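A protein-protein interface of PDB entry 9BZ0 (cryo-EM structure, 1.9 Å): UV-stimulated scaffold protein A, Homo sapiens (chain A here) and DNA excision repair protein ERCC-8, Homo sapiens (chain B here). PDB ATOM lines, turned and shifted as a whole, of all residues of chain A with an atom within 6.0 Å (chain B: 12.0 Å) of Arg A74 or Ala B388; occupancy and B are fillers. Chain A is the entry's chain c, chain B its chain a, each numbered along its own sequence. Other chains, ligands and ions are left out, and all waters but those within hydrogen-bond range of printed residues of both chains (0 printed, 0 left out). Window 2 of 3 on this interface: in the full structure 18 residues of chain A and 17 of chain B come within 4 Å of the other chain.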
ATOM      1  N   LYS A  32     -16.121 -15.947  24.988  1.00  0.00           N
ATOM      2  CA  LYS A  32     -17.355 -16.652  24.660  1.00  0.00           C
ATOM      3  C   LYS A  32     -17.527 -17.920  25.481  1.00  0.00           C
ATOM      4  O   LYS A  32     -18.633 -18.217  25.944  1.00  0.00           O
ATOM      5  CB  LYS A  32     -17.380 -16.989  23.170  1.00  0.00           C
ATOM      6  CG  LYS A  32     -17.636 -15.801  22.266  1.00  0.00           C
ATOM      7  CD  LYS A  32     -17.668 -16.223  20.807  1.00  0.00           C
ATOM      8  CE  LYS A  32     -16.306 -16.706  20.346  1.00  0.00           C
ATOM      9  NZ  LYS A  32     -16.254 -16.916  18.873  1.00  0.00           N
ATOM     10  N   GLU A  69     -21.334  -6.428  20.214  1.00  0.00           N
ATOM     11  CA  GLU A  69     -21.913  -6.892  18.959  1.00  0.00           C
ATOM     12  C   GLU A  69     -21.745  -8.393  18.790  1.00  0.00           C
ATOM     13  O   GLU A  69     -22.669  -9.086  18.351  1.00  0.00           O
ATOM     14  CB  GLU A  69     -21.275  -6.153  17.788  1.00  0.00           C
ATOM     15  CG  GLU A  69     -21.824  -6.539  16.434  1.00  0.00           C
ATOM     16  CD  GLU A  69     -21.112  -5.832  15.297  1.00  0.00           C
ATOM     17  OE1 GLU A  69     -19.942  -5.436  15.483  1.00  0.00           O
ATOM     18  OE2 GLU A  69     -21.720  -5.673  14.219  1.00  0.00           O
ATOM     19  N   GLU A  70     -20.567  -8.909  19.127  1.00  0.00           N
ATOM     20  CA  GLU A  70     -20.320 -10.343  19.038  1.00  0.00           C
ATOM     21  C   GLU A  70     -21.210 -11.144  19.985  1.00  0.00           C
ATOM     22  O   GLU A  70     -21.705 -12.215  19.621  1.00  0.00           O
ATOM     23  CB  GLU A  70     -18.843 -10.605  19.339  1.00  0.00           C
ATOM     24  CG  GLU A  70     -18.390 -12.059  19.351  1.00  0.00           C
ATOM     25  CD  GLU A  70     -18.190 -12.638  17.960  1.00  0.00           C
ATOM     26  OE1 GLU A  70     -18.746 -12.088  16.986  1.00  0.00           O
ATOM     27  OE2 GLU A  70     -17.469 -13.650  17.841  1.00  0.00           O
ATOM     28  N   LEU A  71     -21.439 -10.642  21.196  1.00  0.00           N
ATOM     29  CA  LEU A  71     -22.272 -11.363  22.163  1.00  0.00           C
ATOM     30  C   LEU A  71     -23.778 -11.185  21.972  1.00  0.00           C
ATOM     31  O   LEU A  71     -24.542 -12.106  22.274  1.00  0.00           O
ATOM     32  CB  LEU A  71     -21.892 -10.954  23.580  1.00  0.00           C
ATOM     33  CG  LEU A  71     -20.495 -11.380  24.003  1.00  0.00           C
ATOM     34  CD1 LEU A  71     -20.149 -10.790  25.357  1.00  0.00           C
ATOM     35  CD2 LEU A  71     -20.424 -12.889  24.048  1.00  0.00           C
ATOM     36  N   PHE A  72     -24.224 -10.024  21.502  1.00  0.00           N
ATOM     37  CA  PHE A  72     -25.650  -9.765  21.327  1.00  0.00           C
ATOM     38  C   PHE A  72     -26.283 -10.718  20.323  1.00  0.00           C
ATOM     39  O   PHE A  72     -27.414 -11.173  20.518  1.00  0.00           O
ATOM     40  CB  PHE A  72     -25.835  -8.312  20.882  1.00  0.00           C
ATOM     41  CG  PHE A  72     -27.257  -7.821  20.914  1.00  0.00           C
ATOM     42  CD1 PHE A  72     -28.112  -8.067  19.860  1.00  0.00           C
ATOM     43  CD2 PHE A  72     -27.723  -7.086  21.984  1.00  0.00           C
ATOM     44  CE1 PHE A  72     -29.404  -7.610  19.884  1.00  0.00           C
ATOM     45  CE2 PHE A  72     -29.016  -6.627  22.009  1.00  0.00           C
ATOM     46  CZ  PHE A  72     -29.857  -6.890  20.958  1.00  0.00           C
ATOM     47  N   VAL A  73     -25.566 -11.045  19.253  1.00  0.00           N
ATOM     48  CA  VAL A  73     -26.028 -12.038  18.295  1.00  0.00           C
ATOM     49  C   VAL A  73     -26.158 -13.424  18.920  1.00  0.00           C
ATOM     50  O   VAL A  73     -26.879 -14.277  18.395  1.00  0.00           O
ATOM     51  CB  VAL A  73     -25.066 -12.025  17.090  1.00  0.00           C
ATOM     52  CG1 VAL A  73     -25.335 -13.173  16.131  1.00  0.00           C
ATOM     53  CG2 VAL A  73     -25.159 -10.690  16.374  1.00  0.00           C
ATOM     54  N   ARG A  74     -25.532 -13.651  20.070  1.00  0.00           N
ATOM     55  CA  ARG A  74     -25.314 -14.992  20.587  1.00  0.00           C
ATOM     56  C   ARG A  74     -26.024 -15.342  21.884  1.00  0.00           C
ATOM     57  O   ARG A  74     -26.126 -16.535  22.186  1.00  0.00           O
ATOM     58  CB  ARG A  74     -23.811 -15.256  20.752  1.00  0.00           C
ATOM     59  CG  ARG A  74     -23.118 -15.355  19.414  1.00  0.00           C
ATOM     60  CD  ARG A  74     -21.656 -15.691  19.535  1.00  0.00           C
ATOM     61  NE  ARG A  74     -21.074 -15.900  18.218  1.00  0.00           N
ATOM     62  CZ  ARG A  74     -20.701 -14.923  17.404  1.00  0.00           C
ATOM     63  NH1 ARG A  74     -20.134 -15.228  16.240  1.00  0.00           N
ATOM     64  NH2 ARG A  74     -20.895 -13.654  17.717  1.00  0.00           N
ATOM     65  N   SER A  75     -26.516 -14.383  22.661  1.00  0.00           N
ATOM     66  CA  SER A  75     -27.318 -14.811  23.798  1.00  0.00           C
ATOM     67  C   SER A  75     -28.536 -13.930  24.014  1.00  0.00           C
ATOM     68  O   SER A  75     -28.466 -12.702  23.948  1.00  0.00           O
ATOM     69  CB  SER A  75     -26.486 -14.816  25.079  1.00  0.00           C
ATOM     70  OG  SER A  75     -27.252 -15.277  26.176  1.00  0.00           O
ATOM     71  N   HIS A  76     -29.654 -14.607  24.282  1.00  0.00           N
ATOM     72  CA  HIS A  76     -30.894 -13.958  24.686  1.00  0.00           C
ATOM     73  C   HIS A  76     -30.725 -13.154  25.966  1.00  0.00           C
ATOM     74  O   HIS A  76     -31.249 -12.044  26.081  1.00  0.00           O
ATOM     75  CB  HIS A  76     -31.991 -15.007  24.841  1.00  0.00           C
ATOM     76  CG  HIS A  76     -33.180 -14.534  25.613  1.00  0.00           C
ATOM     77  ND1 HIS A  76     -33.256 -14.615  26.987  1.00  0.00           N
ATOM     78  CD2 HIS A  76     -34.350 -13.991  25.203  1.00  0.00           C
ATOM     79  CE1 HIS A  76     -34.417 -14.130  27.390  1.00  0.00           C
ATOM     80  NE2 HIS A  76     -35.100 -13.745  26.327  1.00  0.00           N
ATOM     81  N   ARG A  79     -28.865 -10.021  25.168  1.00  0.00           N
ATOM     82  CA  ARG A  79     -29.782  -9.114  24.489  1.00  0.00           C
ATOM     83  C   ARG A  79     -30.727  -8.435  25.469  1.00  0.00           C
ATOM     84  O   ARG A  79     -30.943  -7.221  25.399  1.00  0.00           O
ATOM     85  CB  ARG A  79     -30.582  -9.877  23.440  1.00  0.00           C
ATOM     86  CG  ARG A  79     -29.793 -10.278  22.234  1.00  0.00           C
ATOM     87  CD  ARG A  79     -30.702 -10.811  21.149  1.00  0.00           C
ATOM     88  NE  ARG A  79     -31.303 -12.084  21.522  1.00  0.00           N
ATOM     89  CZ  ARG A  79     -30.771 -13.270  21.265  1.00  0.00           C
ATOM     90  NH1 ARG A  79     -31.474 -14.366  21.533  1.00  0.00           N
ATOM     91  NH2 ARG A  79     -29.542 -13.388  20.795  1.00  0.00           N
ATOM     92  N   LEU B 381     -41.934 -20.643  20.052  1.00  0.00           N
ATOM     93  CA  LEU B 381     -40.609 -20.299  20.571  1.00  0.00           C
ATOM     94  C   LEU B 381     -39.824 -19.606  19.461  1.00  0.00           C
ATOM     95  O   LEU B 381     -39.008 -20.208  18.756  1.00  0.00           O
ATOM     96  CB  LEU B 381     -39.891 -21.542  21.081  1.00  0.00           C
ATOM     97  CG  LEU B 381     -40.547 -22.272  22.255  1.00  0.00           C
ATOM     98  CD1 LEU B 381     -39.819 -23.574  22.551  1.00  0.00           C
ATOM     99  CD2 LEU B 381     -40.588 -21.383  23.488  1.00  0.00           C
ATOM    100  N   ASN B 382     -40.104 -18.317  19.294  1.00  0.00           N
ATOM    101  CA  ASN B 382     -39.449 -17.531  18.259  1.00  0.00           C
ATOM    102  C   ASN B 382     -37.931 -17.601  18.415  1.00  0.00           C
ATOM    103  O   ASN B 382     -37.411 -17.497  19.533  1.00  0.00           O
ATOM    104  CB  ASN B 382     -39.926 -16.077  18.332  1.00  0.00           C
ATOM    105  CG  ASN B 382     -39.428 -15.229  17.174  1.00  0.00           C
ATOM    106  OD1 ASN B 382     -38.226 -15.041  16.991  1.00  0.00           O
ATOM    107  ND2 ASN B 382     -40.361 -14.709  16.383  1.00  0.00           N
ATOM    108  N   PRO B 383     -37.196 -17.783  17.317  1.00  0.00           N
ATOM    109  CA  PRO B 383     -35.732 -17.912  17.407  1.00  0.00           C
ATOM    110  C   PRO B 383     -35.020 -16.683  17.948  1.00  0.00           C
ATOM    111  O   PRO B 383     -33.854 -16.793  18.347  1.00  0.00           O
ATOM    112  CB  PRO B 383     -35.313 -18.209  15.959  1.00  0.00           C
ATOM    113  CG  PRO B 383     -36.437 -17.699  15.118  1.00  0.00           C
ATOM    114  CD  PRO B 383     -37.677 -17.917  15.934  1.00  0.00           C
ATOM    115  N   ALA B 384     -35.671 -15.518  17.975  1.00  0.00           N
ATOM    116  CA  ALA B 384     -35.093 -14.373  18.664  1.00  0.00           C
ATOM    117  C   ALA B 384     -34.875 -14.625  20.150  1.00  0.00           C
ATOM    118  O   ALA B 384     -34.041 -13.952  20.762  1.00  0.00           O
ATOM    119  CB  ALA B 384     -35.984 -13.145  18.473  1.00  0.00           C
ATOM    120  N   PHE B 385     -35.594 -15.569  20.739  1.00  0.00           N
ATOM    121  CA  PHE B 385     -35.387 -15.938  22.132  1.00  0.00           C
ATOM    122  C   PHE B 385     -34.305 -16.993  22.312  1.00  0.00           C
ATOM    123  O   PHE B 385     -34.055 -17.410  23.446  1.00  0.00           O
ATOM    124  CB  PHE B 385     -36.696 -16.437  22.747  1.00  0.00           C
ATOM    125  CG  PHE B 385     -37.847 -15.490  22.571  1.00  0.00           C
ATOM    126  CD1 PHE B 385     -37.707 -14.146  22.871  1.00  0.00           C
ATOM    127  CD2 PHE B 385     -39.069 -15.944  22.104  1.00  0.00           C
ATOM    128  CE1 PHE B 385     -38.765 -13.272  22.711  1.00  0.00           C
ATOM    129  CE2 PHE B 385     -40.131 -15.075  21.940  1.00  0.00           C
ATOM    130  CZ  PHE B 385     -39.978 -13.737  22.244  1.00  0.00           C
ATOM    131  N   GLU B 386     -33.655 -17.428  21.236  1.00  0.00           N
ATOM    132  CA  GLU B 386     -32.716 -18.539  21.290  1.00  0.00           C
ATOM    133  C   GLU B 386     -31.271 -18.054  21.287  1.00  0.00           C
ATOM    134  O   GLU B 386     -30.933 -17.065  20.632  1.00  0.00           O
ATOM    135  CB  GLU B 386     -32.938 -19.486  20.109  1.00  0.00           C
ATOM    136  CG  GLU B 386     -34.309 -20.143  20.084  1.00  0.00           C
ATOM    137  CD  GLU B 386     -34.369 -21.327  19.139  1.00  0.00           C
ATOM    138  OE1 GLU B 386     -33.869 -21.205  18.002  1.00  0.00           O
ATOM    139  OE2 GLU B 386     -34.917 -22.378  19.531  1.00  0.00           O
ATOM    140  N   ASP B 387     -30.428 -18.773  22.022  1.00  0.00           N
ATOM    141  CA  ASP B 387     -28.981 -18.650  21.971  1.00  0.00           C
ATOM    142  C   ASP B 387     -28.419 -19.330  20.728  1.00  0.00           C
ATOM    143  O   ASP B 387     -29.056 -20.190  20.115  1.00  0.00           O
ATOM    144  CB  ASP B 387     -28.353 -19.255  23.225  1.00  0.00           C
ATOM    145  CG  ASP B 387     -28.959 -18.709  24.499  1.00  0.00           C
ATOM    146  OD1 ASP B 387     -28.958 -17.474  24.678  1.00  0.00           O
ATOM    147  OD2 ASP B 387     -29.441 -19.515  25.322  1.00  0.00           O
ATOM    148  N   ALA B 388     -27.210 -18.927  20.353  1.00  0.00           N
ATOM    149  CA  ALA B 388     -26.623 -19.340  19.083  1.00  0.00           C
ATOM    150  C   ALA B 388     -25.102 -19.409  19.209  1.00  0.00           C
ATOM    151  O   ALA B 388     -24.362 -18.895  18.370  1.00  0.00           O
ATOM    152  CB  ALA B 388     -27.050 -18.400  17.957  1.00  0.00           C
ATOM    153  N   TRP B 389     -24.616 -20.058  20.271  1.00  0.00           N
ATOM    154  CA  TRP B 389     -23.190 -20.060  20.582  1.00  0.00           C
ATOM    155  C   TRP B 389     -22.332 -20.713  19.507  1.00  0.00           C
ATOM    156  O   TRP B 389     -21.104 -20.583  19.560  1.00  0.00           O
ATOM    157  CB  TRP B 389     -22.936 -20.777  21.908  1.00  0.00           C
ATOM    158  CG  TRP B 389     -23.654 -20.196  23.067  1.00  0.00           C
ATOM    159  CD1 TRP B 389     -24.711 -20.737  23.729  1.00  0.00           C
ATOM    160  CD2 TRP B 389     -23.347 -18.969  23.732  1.00  0.00           C
ATOM    161  NE1 TRP B 389     -25.095 -19.916  24.758  1.00  0.00           N
ATOM    162  CE2 TRP B 389     -24.271 -18.822  24.781  1.00  0.00           C
ATOM    163  CE3 TRP B 389     -22.386 -17.976  23.538  1.00  0.00           C
ATOM    164  CZ2 TRP B 389     -24.263 -17.723  25.632  1.00  0.00           C
ATOM    165  CZ3 TRP B 389     -22.378 -16.887  24.383  1.00  0.00           C
ATOM    166  CH2 TRP B 389     -23.309 -16.768  25.418  1.00  0.00           C
ATOM    167  N   SER B 390     -22.930 -21.414  18.550  1.00  0.00           N
ATOM    168  CA  SER B 390     -22.166 -22.085  17.504  1.00  0.00           C
ATOM    169  C   SER B 390     -21.359 -21.092  16.672  1.00  0.00           C
ATOM    170  O   SER B 390     -21.917 -20.177  16.068  1.00  0.00           O
ATOM    171  CB  SER B 390     -23.097 -22.891  16.597  1.00  0.00           C
ATOM    172  OG  SER B 390     -22.363 -23.613  15.624  1.00  0.00           O
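Hydrophobic or aromatic side chains of chain B within 4 Å of the printed part of chain A: Trp B389.
Hydrophobic or aromatic side chains of chain A that line the printed part of chain B: His A76.
Among the printed residues, 10 pairs touch across the chains.
Among the printed residues, no Asp or Glu carboxylate lies within 4 Å of a Lys or Arg side-chain nitrogen of the other chain.
The guanidinium group of Arg A79 sits at hydrogen-bond distance from the backbone carbonyl oxygen of Ala B384 (2.7 Å).
N of Ala B388 sits at hydrogen-bond distance from O of Arg A74, at 3.2 Å.
OD1 of Asp B387 lies within hydrogen-bond range of N of His A76.
OG of Ser A75 is in hydrogen-bond range of OD1 of Asp B387.
O of Glu B386 sits at hydrogen-bond distance from NH1 of Arg A79.
Among the printed residues, merely in contact across the chains: His A76 with Phe B385 (3.5 Å), Arg A74 with Asp B387 (3.6 Å), Ser A75 with Trp B389 (3.7 Å), Arg A74 with Trp B389 (3.9 Å) and Arg A79 with Phe B385 (3.9 Å).
O of Ser A75 lies close to NH2 of Arg A79, at 3.4 Å.
The guanidinium group (NH2) of Arg A79 sits close to the backbone carbonyl oxygen (O) of Phe A72, 3.1 Å away.
OE1 of Glu A70 lies within salt-bridge range of NH2 of Arg A74.
The side-chain amide oxygen (OD1) of Asn B382 sits at hydrogen-bond distance from the backbone NH (N) of Ala B384 (2.8 Å).
Of chain B, only Asp B387 (3.6 Å), Ala B388 (3.2 Å) and Trp B389 (3.9 Å) come within 4 Å of Arg A74.
Of the printed residues of chain A, Ala B388 touches Arg A74 (3.2 Å).
No residue of chain B comes within 4 Å of Glu A70.
No residue of chain B comes within 4 Å of Val A73.
Of chain B, only Asp B387 (3.2 Å) and Trp B389 (3.7 Å) come within 4 Å of Ser A75.
Printed residues of chain A within 4 Å of Trp B389: Arg A74 and Ser A75.
Printed residues of chain B within 4 Å of Arg A79: Ala B384 (2.7 Å), Phe B385 (3.9 Å) and Glu B386 (2.9 Å).
Printed residues of chain A within 4 Å of Glu B386: Arg A79 (2.9 Å).
Of the printed residues of chain B, His A76 touches Phe B385 and Asp B387.
Phe A72 touches none of the printed residues of chain B.
Asn B382 touches none of the printed residues of chain A.
The nearest residue of chain A that does not touch Ala B388 is Val A73 (4.1 Å).
The nearest printed residue of chain A that does not touch Asp B387 is Arg A79 (4.6 Å).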
